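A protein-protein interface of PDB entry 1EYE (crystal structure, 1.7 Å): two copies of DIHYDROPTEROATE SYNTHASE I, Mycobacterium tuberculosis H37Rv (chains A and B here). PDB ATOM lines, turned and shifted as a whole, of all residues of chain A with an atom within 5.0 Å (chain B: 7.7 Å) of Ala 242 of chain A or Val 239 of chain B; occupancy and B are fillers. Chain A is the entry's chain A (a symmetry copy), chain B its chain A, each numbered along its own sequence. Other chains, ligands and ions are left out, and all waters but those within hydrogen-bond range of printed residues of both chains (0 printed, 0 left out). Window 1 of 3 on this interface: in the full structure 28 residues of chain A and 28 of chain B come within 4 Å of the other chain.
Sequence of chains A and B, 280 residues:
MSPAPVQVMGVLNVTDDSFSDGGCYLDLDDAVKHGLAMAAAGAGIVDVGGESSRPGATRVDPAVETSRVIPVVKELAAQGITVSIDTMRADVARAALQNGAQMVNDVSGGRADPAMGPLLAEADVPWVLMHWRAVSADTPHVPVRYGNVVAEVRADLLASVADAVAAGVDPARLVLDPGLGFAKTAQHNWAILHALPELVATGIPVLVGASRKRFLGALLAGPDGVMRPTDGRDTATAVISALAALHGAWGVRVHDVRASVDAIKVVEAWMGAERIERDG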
ATOM      1  N   ALA A 238      31.018  -8.329  22.182  1.00  0.00           N
ATOM      2  CA  ALA A 238      30.289  -8.698  20.979  1.00  0.00           C
ATOM      3  C   ALA A 238      28.770  -8.532  21.154  1.00  0.00           C
ATOM      4  O   ALA A 238      28.062  -8.075  20.257  1.00  0.00           O
ATOM      5  CB  ALA A 238      30.663 -10.127  20.566  1.00  0.00           C
ATOM      6  N   VAL A 239      28.279  -8.884  22.341  1.00  0.00           N
ATOM      7  CA  VAL A 239      26.876  -8.755  22.655  1.00  0.00           C
ATOM      8  C   VAL A 239      26.503  -7.292  22.720  1.00  0.00           C
ATOM      9  O   VAL A 239      25.446  -6.897  22.286  1.00  0.00           O
ATOM     10  CB  VAL A 239      26.531  -9.503  23.942  1.00  0.00           C
ATOM     11  CG1 VAL A 239      25.077  -9.213  24.288  1.00  0.00           C
ATOM     12  CG2 VAL A 239      26.677 -10.996  23.639  1.00  0.00           C
ATOM     13  N   ILE A 240      27.393  -6.482  23.256  1.00  0.00           N
ATOM     14  CA  ILE A 240      27.114  -5.048  23.283  1.00  0.00           C
ATOM     15  C   ILE A 240      27.047  -4.547  21.836  1.00  0.00           C
ATOM     16  O   ILE A 240      26.236  -3.700  21.486  1.00  0.00           O
ATOM     17  CB  ILE A 240      28.131  -4.281  24.123  1.00  0.00           C
ATOM     18  CG1 ILE A 240      27.739  -4.416  25.597  1.00  0.00           C
ATOM     19  CG2 ILE A 240      28.142  -2.801  23.683  1.00  0.00           C
ATOM     20  CD1 ILE A 240      28.874  -4.100  26.568  1.00  0.00           C
ATOM     21  N   SER A 241      27.865  -5.121  20.943  1.00  0.00           N
ATOM     22  CA  SER A 241      27.805  -4.737  19.526  1.00  0.00           C
ATOM     23  C   SER A 241      26.433  -5.052  18.895  1.00  0.00           C
ATOM     24  O   SER A 241      25.824  -4.246  18.171  1.00  0.00           O
ATOM     25  CB  SER A 241      28.913  -5.372  18.694  1.00  0.00           C
ATOM     26  OG  SER A 241      30.167  -4.860  19.103  1.00  0.00           O
ATOM     27  N   ALA A 242      25.918  -6.256  19.176  1.00  0.00           N
ATOM     28  CA  ALA A 242      24.596  -6.618  18.644  1.00  0.00           C
ATOM     29  C   ALA A 242      23.499  -5.679  19.158  1.00  0.00           C
ATOM     30  O   ALA A 242      22.610  -5.261  18.425  1.00  0.00           O
ATOM     31  CB  ALA A 242      24.232  -8.043  19.081  1.00  0.00           C
ATOM     32  N   LEU A 243      23.521  -5.390  20.470  1.00  0.00           N
ATOM     33  CA  LEU A 243      22.500  -4.534  21.052  1.00  0.00           C
ATOM     34  C   LEU A 243      22.649  -3.137  20.480  1.00  0.00           C
ATOM     35  O   LEU A 243      21.682  -2.437  20.243  1.00  0.00           O
ATOM     36  CB  LEU A 243      22.595  -4.467  22.586  1.00  0.00           C
ATOM     37  CG  LEU A 243      21.540  -5.312  23.315  1.00  0.00           C
ATOM     38  CD1 LEU A 243      21.131  -6.471  22.444  1.00  0.00           C
ATOM     39  CD2 LEU A 243      22.042  -5.844  24.649  1.00  0.00           C
ATOM     40  N   ALA A 244      23.889  -2.729  20.261  1.00  0.00           N
ATOM     41  CA  ALA A 244      24.117  -1.404  19.710  1.00  0.00           C
ATOM     42  C   ALA A 244      23.537  -1.323  18.308  1.00  0.00           C
ATOM     43  O   ALA A 244      22.909  -0.335  17.913  1.00  0.00           O
ATOM     44  CB  ALA A 244      25.603  -1.089  19.673  1.00  0.00           C
ATOM     45  N   ALA A 245      23.747  -2.409  17.568  1.00  0.00           N
ATOM     46  CA  ALA A 245      23.231  -2.494  16.216  1.00  0.00           C
ATOM     47  C   ALA A 245      21.704  -2.388  16.221  1.00  0.00           C
ATOM     48  O   ALA A 245      21.089  -1.661  15.435  1.00  0.00           O
ATOM     49  CB  ALA A 245      23.711  -3.770  15.547  1.00  0.00           C
ATOM     50  N   LEU A 246      21.095  -3.119  17.143  1.00  0.00           N
ATOM     51  CA  LEU A 246      19.653  -3.120  17.307  1.00  0.00           C
ATOM     52  C   LEU A 246      19.084  -1.745  17.672  1.00  0.00           C
ATOM     53  O   LEU A 246      17.925  -1.427  17.418  1.00  0.00           O
ATOM     54  CB  LEU A 246      19.291  -4.032  18.493  1.00  0.00           C
ATOM     55  CG  LEU A 246      19.252  -5.494  18.128  1.00  0.00           C
ATOM     56  CD1 LEU A 246      18.874  -6.281  19.390  1.00  0.00           C
ATOM     57  CD2 LEU A 246      18.222  -5.696  17.006  1.00  0.00           C
ATOM     58  N   ALA A 263      28.737 -11.108  15.684  1.00  0.00           N
ATOM     59  CA  ALA A 263      27.530 -10.631  16.349  1.00  0.00           C
ATOM     60  C   ALA A 263      26.614  -9.878  15.412  1.00  0.00           C
ATOM     61  O   ALA A 263      25.399 -10.050  15.435  1.00  0.00           O
ATOM     62  CB  ALA A 263      27.841  -9.777  17.577  1.00  0.00           C
ATOM     63  N   VAL A 266      24.880 -12.078  12.959  1.00  0.00           N
ATOM     64  CA  VAL A 266      23.746 -12.742  13.604  1.00  0.00           C
ATOM     65  C   VAL A 266      22.520 -11.822  13.634  1.00  0.00           C
ATOM     66  O   VAL A 266      21.392 -12.186  13.279  1.00  0.00           O
ATOM     67  CB  VAL A 266      24.048 -13.245  15.041  1.00  0.00           C
ATOM     68  CG1 VAL A 266      22.766 -13.735  15.743  1.00  0.00           C
ATOM     69  CG2 VAL A 266      25.052 -14.413  15.033  1.00  0.00           C
ATOM     70  N   VAL A 267      22.740 -10.601  14.111  1.00  0.00           N
ATOM     71  CA  VAL A 267      21.654  -9.657  14.221  1.00  0.00           C
ATOM     72  C   VAL A 267      21.000  -9.461  12.871  1.00  0.00           C
ATOM     73  O   VAL A 267      19.779  -9.461  12.742  1.00  0.00           O
ATOM     74  CB  VAL A 267      22.120  -8.312  14.757  1.00  0.00           C
ATOM     75  CG1 VAL A 267      20.939  -7.363  14.659  1.00  0.00           C
ATOM     76  CG2 VAL A 267      22.520  -8.481  16.208  1.00  0.00           C
ATOM     77  N   ARG B 233      32.061 -20.981  16.635  1.00  0.00           N
ATOM     78  CA  ARG B 233      30.678 -20.549  16.517  1.00  0.00           C
ATOM     79  C   ARG B 233      30.094 -20.110  17.839  1.00  0.00           C
ATOM     80  O   ARG B 233      28.895 -19.868  17.919  1.00  0.00           O
ATOM     81  CB  ARG B 233      29.787 -21.664  15.935  1.00  0.00           C
ATOM     82  CG  ARG B 233      30.328 -22.178  14.616  1.00  0.00           C
ATOM     83  CD  ARG B 233      29.682 -23.469  14.113  1.00  0.00           C
ATOM     84  NE  ARG B 233      30.443 -24.081  12.997  1.00  0.00           N
ATOM     85  CZ  ARG B 233      30.077 -25.218  12.391  1.00  0.00           C
ATOM     86  NH1 ARG B 233      28.971 -25.874  12.742  1.00  0.00           N
ATOM     87  NH2 ARG B 233      30.809 -25.700  11.398  1.00  0.00           N
ATOM     88  N   ASP B 234      30.906 -20.010  18.881  1.00  0.00           N
ATOM     89  CA  ASP B 234      30.346 -19.614  20.166  1.00  0.00           C
ATOM     90  C   ASP B 234      29.893 -18.175  20.288  1.00  0.00           C
ATOM     91  O   ASP B 234      28.891 -17.916  20.932  1.00  0.00           O
ATOM     92  CB  ASP B 234      31.219 -20.019  21.354  1.00  0.00           C
ATOM     93  CG  ASP B 234      31.304 -21.523  21.452  1.00  0.00           C
ATOM     94  OD1 ASP B 234      30.366 -22.270  21.223  1.00  0.00           O
ATOM     95  OD2 ASP B 234      32.502 -21.923  21.785  1.00  0.00           O
ATOM     96  N   THR B 235      30.617 -17.234  19.691  1.00  0.00           N
ATOM     97  CA  THR B 235      30.161 -15.853  19.805  1.00  0.00           C
ATOM     98  C   THR B 235      28.768 -15.735  19.195  1.00  0.00           C
ATOM     99  O   THR B 235      27.853 -15.165  19.803  1.00  0.00           O
ATOM    100  CB  THR B 235      31.144 -14.817  19.183  1.00  0.00           C
ATOM    101  OG1 THR B 235      32.420 -15.054  19.713  1.00  0.00           O
ATOM    102  CG2 THR B 235      30.708 -13.418  19.575  1.00  0.00           C
ATOM    103  N   ALA B 236      28.617 -16.274  17.990  1.00  0.00           N
ATOM    104  CA  ALA B 236      27.314 -16.253  17.316  1.00  0.00           C
ATOM    105  C   ALA B 236      26.243 -16.910  18.178  1.00  0.00           C
ATOM    106  O   ALA B 236      25.108 -16.411  18.323  1.00  0.00           O
ATOM    107  CB  ALA B 236      27.400 -16.906  15.940  1.00  0.00           C
ATOM    108  N   THR B 237      26.639 -18.046  18.780  1.00  0.00           N
ATOM    109  CA  THR B 237      25.726 -18.757  19.662  1.00  0.00           C
ATOM    110  C   THR B 237      25.314 -17.866  20.836  1.00  0.00           C
ATOM    111  O   THR B 237      24.150 -17.793  21.204  1.00  0.00           O
ATOM    112  CB  THR B 237      26.349 -20.045  20.205  1.00  0.00           C
ATOM    113  OG1 THR B 237      26.637 -20.926  19.131  1.00  0.00           O
ATOM    114  CG2 THR B 237      25.337 -20.676  21.158  1.00  0.00           C
ATOM    115  N   ALA B 238      26.302 -17.196  21.439  1.00  0.00           N
ATOM    116  CA  ALA B 238      26.066 -16.308  22.567  1.00  0.00           C
ATOM    117  C   ALA B 238      25.125 -15.150  22.198  1.00  0.00           C
ATOM    118  O   ALA B 238      24.252 -14.755  22.971  1.00  0.00           O
ATOM    119  CB  ALA B 238      27.408 -15.802  23.114  1.00  0.00           C
ATOM    120  N   VAL B 239      25.295 -14.624  20.986  1.00  0.00           N
ATOM    121  CA  VAL B 239      24.464 -13.550  20.496  1.00  0.00           C
ATOM    122  C   VAL B 239      23.053 -14.053  20.291  1.00  0.00           C
ATOM    123  O   VAL B 239      22.098 -13.365  20.567  1.00  0.00           O
ATOM    124  CB  VAL B 239      25.053 -12.934  19.229  1.00  0.00           C
ATOM    125  CG1 VAL B 239      24.065 -11.909  18.691  1.00  0.00           C
ATOM    126  CG2 VAL B 239      26.336 -12.211  19.644  1.00  0.00           C
ATOM    127  N   ILE B 240      22.929 -15.276  19.816  1.00  0.00           N
ATOM    128  CA  ILE B 240      21.589 -15.837  19.661  1.00  0.00           C
ATOM    129  C   ILE B 240      20.961 -15.964  21.054  1.00  0.00           C
ATOM    130  O   ILE B 240      19.775 -15.736  21.247  1.00  0.00           O
ATOM    131  CB  ILE B 240      21.606 -17.161  18.903  1.00  0.00           C
ATOM    132  CG1 ILE B 240      21.684 -16.857  17.404  1.00  0.00           C
ATOM    133  CG2 ILE B 240      20.329 -17.959  19.243  1.00  0.00           C
ATOM    134  CD1 ILE B 240      22.155 -18.038  16.559  1.00  0.00           C
ATOM    135  N   SER B 241      21.774 -16.268  22.075  1.00  0.00           N
ATOM    136  CA  SER B 241      21.251 -16.338  23.446  1.00  0.00           C
ATOM    137  C   SER B 241      20.690 -14.983  23.926  1.00  0.00           C
ATOM    138  O   SER B 241      19.602 -14.875  24.516  1.00  0.00           O
ATOM    139  CB  SER B 241      22.279 -16.853  24.446  1.00  0.00           C
ATOM    140  OG  SER B 241      22.584 -18.206  24.160  1.00  0.00           O
ATOM    141  N   ALA B 242      21.445 -13.909  23.663  1.00  0.00           N
ATOM    142  CA  ALA B 242      20.963 -12.576  24.054  1.00  0.00           C
ATOM    143  C   ALA B 242      19.650 -12.217  23.350  1.00  0.00           C
ATOM    144  O   ALA B 242      18.731 -11.661  23.941  1.00  0.00           O
ATOM    145  CB  ALA B 242      22.003 -11.514  23.670  1.00  0.00           C
ATOM    146  N   LEU B 243      19.581 -12.480  22.034  1.00  0.00           N
ATOM    147  CA  LEU B 243      18.385 -12.142  21.279  1.00  0.00           C
ATOM    148  C   LEU B 243      17.236 -13.001  21.772  1.00  0.00           C
ATOM    149  O   LEU B 243      16.100 -12.569  21.844  1.00  0.00           O
ATOM    150  CB  LEU B 243      18.568 -12.358  19.767  1.00  0.00           C
ATOM    151  CG  LEU B 243      18.785 -11.062  18.972  1.00  0.00           C
ATOM    152  CD1 LEU B 243      19.420 -10.026  19.860  1.00  0.00           C
ATOM    153  CD2 LEU B 243      19.661 -11.273  17.746  1.00  0.00           C
ATOM    154  N   ALA B 244      17.544 -14.243  22.113  1.00  0.00           N
ATOM    155  CA  ALA B 244      16.501 -15.128  22.600  1.00  0.00           C
ATOM    156  C   ALA B 244      15.948 -14.599  23.913  1.00  0.00           C
ATOM    157  O   ALA B 244      14.738 -14.598  24.164  1.00  0.00           O
ATOM    158  CB  ALA B 244      17.042 -16.535  22.796  1.00  0.00           C
ATOM    159  N   ALA B 245      16.876 -14.126  24.742  1.00  0.00           N
ATOM    160  CA  ALA B 245      16.502 -13.561  26.024  1.00  0.00           C
ATOM    161  C   ALA B 245      15.585 -12.352  25.827  1.00  0.00           C
ATOM    162  O   ALA B 245      14.552 -12.191  26.484  1.00  0.00           O
ATOM    163  CB  ALA B 245      17.741 -13.211  26.828  1.00  0.00           C
ATOM    164  N   LEU B 246      15.973 -11.502  24.887  1.00  0.00           N
ATOM    165  CA  LEU B 246      15.211 -10.314  24.550  1.00  0.00           C
ATOM    166  C   LEU B 246      13.803 -10.625  24.031  1.00  0.00           C
ATOM    167  O   LEU B 246      12.879  -9.822  24.121  1.00  0.00           O
ATOM    168  CB  LEU B 246      15.916  -9.587  23.391  1.00  0.00           C
ATOM    169  CG  LEU B 246      17.065  -8.723  23.844  1.00  0.00           C
ATOM    170  CD1 LEU B 246      17.666  -8.056  22.599  1.00  0.00           C
ATOM    171  CD2 LEU B 246      16.537  -7.681  24.843  1.00  0.00           C
ATOM    172  N   ALA B 259      30.127 -18.342  27.618  1.00  0.00           N
ATOM    173  CA  ALA B 259      29.767 -17.413  26.565  1.00  0.00           C
ATOM    174  C   ALA B 259      28.294 -16.990  26.617  1.00  0.00           C
ATOM    175  O   ALA B 259      27.978 -15.791  26.574  1.00  0.00           O
ATOM    176  CB  ALA B 259      30.258 -17.916  25.214  1.00  0.00           C
ATOM    177  N   SER B 260      27.378 -17.964  26.723  1.00  0.00           N
ATOM    178  CA  SER B 260      25.970 -17.612  26.782  1.00  0.00           C
ATOM    179  C   SER B 260      25.593 -16.933  28.091  1.00  0.00           C
ATOM    180  O   SER B 260      24.732 -16.066  28.125  1.00  0.00           O
ATOM    181  CB  SER B 260      25.025 -18.755  26.386  1.00  0.00           C
ATOM    182  OG  SER B 260      25.071 -18.951  24.973  1.00  0.00           O
ATOM    183  N   ALA B 263      26.585 -13.342  27.780  1.00  0.00           N
ATOM    184  CA  ALA B 263      25.613 -12.646  26.944  1.00  0.00           C
ATOM    185  C   ALA B 263      24.377 -12.240  27.713  1.00  0.00           C
ATOM    186  O   ALA B 263      23.862 -11.136  27.554  1.00  0.00           O
ATOM    187  CB  ALA B 263      25.221 -13.456  25.710  1.00  0.00           C
ATOM    188  N   VAL B 267      22.716  -8.536  28.579  1.00  0.00           N
ATOM    189  CA  VAL B 267      21.354  -8.163  28.277  1.00  0.00           C
ATOM    190  C   VAL B 267      20.673  -7.640  29.521  1.00  0.00           C
ATOM    191  O   VAL B 267      19.994  -6.617  29.501  1.00  0.00           O
ATOM    192  CB  VAL B 267      20.555  -9.328  27.714  1.00  0.00           C
ATOM    193  CG1 VAL B 267      19.113  -8.865  27.606  1.00  0.00           C
ATOM    194  CG2 VAL B 267      21.089  -9.662  26.336  1.00  0.00           C
ATOM    195  N   TRP B 270      22.089  -4.273  30.478  1.00  0.00           N
ATOM    196  CA  TRP B 270      21.634  -3.239  29.580  1.00  0.00           C
ATOM    197  C   TRP B 270      20.157  -2.944  29.763  1.00  0.00           C
ATOM    198  O   TRP B 270      19.728  -1.810  29.978  1.00  0.00           O
ATOM    199  CB  TRP B 270      21.928  -3.656  28.136  1.00  0.00           C
ATOM    200  CG  TRP B 270      21.549  -2.715  27.024  1.00  0.00           C
ATOM    201  CD1 TRP B 270      20.339  -2.155  26.785  1.00  0.00           C
ATOM    202  CD2 TRP B 270      22.392  -2.308  25.929  1.00  0.00           C
ATOM    203  NE1 TRP B 270      20.390  -1.383  25.639  1.00  0.00           N
ATOM    204  CE2 TRP B 270      21.635  -1.476  25.085  1.00  0.00           C
ATOM    205  CE3 TRP B 270      23.713  -2.571  25.582  1.00  0.00           C
ATOM    206  CZ2 TRP B 270      22.168  -0.913  23.917  1.00  0.00           C
ATOM    207  CZ3 TRP B 270      24.230  -2.018  24.431  1.00  0.00           C
ATOM    208  CH2 TRP B 270      23.472  -1.185  23.611  1.00  0.00           C
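Among the printed residues, pairs that only touch across the chains: Ala 238 of chain A with Thr 235 of chain B (3.4 Å), Leu 243 of chain A with Trp 270 of chain B (3.5 Å), Val 239 of chain A with Ala 263 of chain B (3.5 Å), Ala 263 of chain A with Val 239 of chain B (3.5 Å), Val 266 of chain A with Ala 236 of chain B (3.5 Å), Val 266 of chain A with Ile 240 of chain B (3.7 Å), Val 266 of chain A with Val 239 of chain B (3.7 Å), Ala 244 of chain A with Trp 270 of chain B (3.7 Å), Leu 243 of chain A with Leu 246 of chain B (3.8 Å), Leu 246 of chain A with Leu 243 of chain B (3.8 Å), Leu 246 of chain A with Leu 246 of chain B (3.9 Å), Ala 242 of chain A with Val 239 of chain B (3.9 Å), Val 239 of chain A with Ala 242 of chain B (3.9 Å) and Ile 240 of chain A with Trp 270 of chain B (3.9 Å).
Printed residues of chain B within 4 Å of Ala 238 of chain A: Thr 235 (3.4 Å). Of the printed residues of chain B, Ile 240 of chain A touches Trp 270 (3.9 Å). Ala 242 of chain A touches just one residue of chain B: Val 239. Ala 245 of chain A touches none of the printed residues of chain B. Thr 237 of chain B touches none of the printed residues of chain A. Printed residues of chain A within 4 Å of Val 239 of chain B: Ala 242, Ala 263 and Val 266. Of the printed residues of chain A, Leu 243 of chain B touches Leu 246. Printed residues of chain A within 4 Å of Leu 246 of chain B: Leu 243 and Leu 246. The nearest residue of chain B that does not touch Ala 242 of chain A is Leu 243 of chain B (5.3 Å). The nearest residue of chain A that does not touch Val 239 of chain B is Val 239 of chain A (4.2 Å).
Of the 12 printed residues of chain A, 9 touch a printed residue of chain B. Hydrophobic or aromatic side chains of chain A that line the printed part of chain B: Ala 238, Val 239, Ala 242, Leu 243, Leu 246, Ala 263 and Val 266. Of the 19 printed residues of chain B, 9 touch a printed residue of chain A. Hydrophobic or aromatic side chains of chain B within 4 Å of the printed part of chain A: Ala 236, Val 239, Ile 240, Ala 242, Leu 243, Leu 246, Ala 263 and Trp 270. Among the printed residues, 14 pairs touch across the chains. Among the printed residues, no Asp or Glu carboxylate lies within 4 Å of a Lys or Arg side-chain nitrogen of the other chain.
Val 239 of chain A touches Ala 242 of chain B, and with the chains exchanged Ala 242 of chain A touches Val 239 of chain B. Val 239 of chain A touches Ala 263 of chain B, and with the chains exchanged Ala 263 of chain A touches Val 239 of chain B. Leu 243 of chain A touches Leu 246 of chain B, and with the chains exchanged Leu 246 of chain A touches Leu 243 of chain B. Leu 246 of chain B touches its own counterpart, Leu 246 of chain A. Of the 14 pairs that touch across the chains among the printed residues, 7 have their exchanged pair printed and touching as well.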
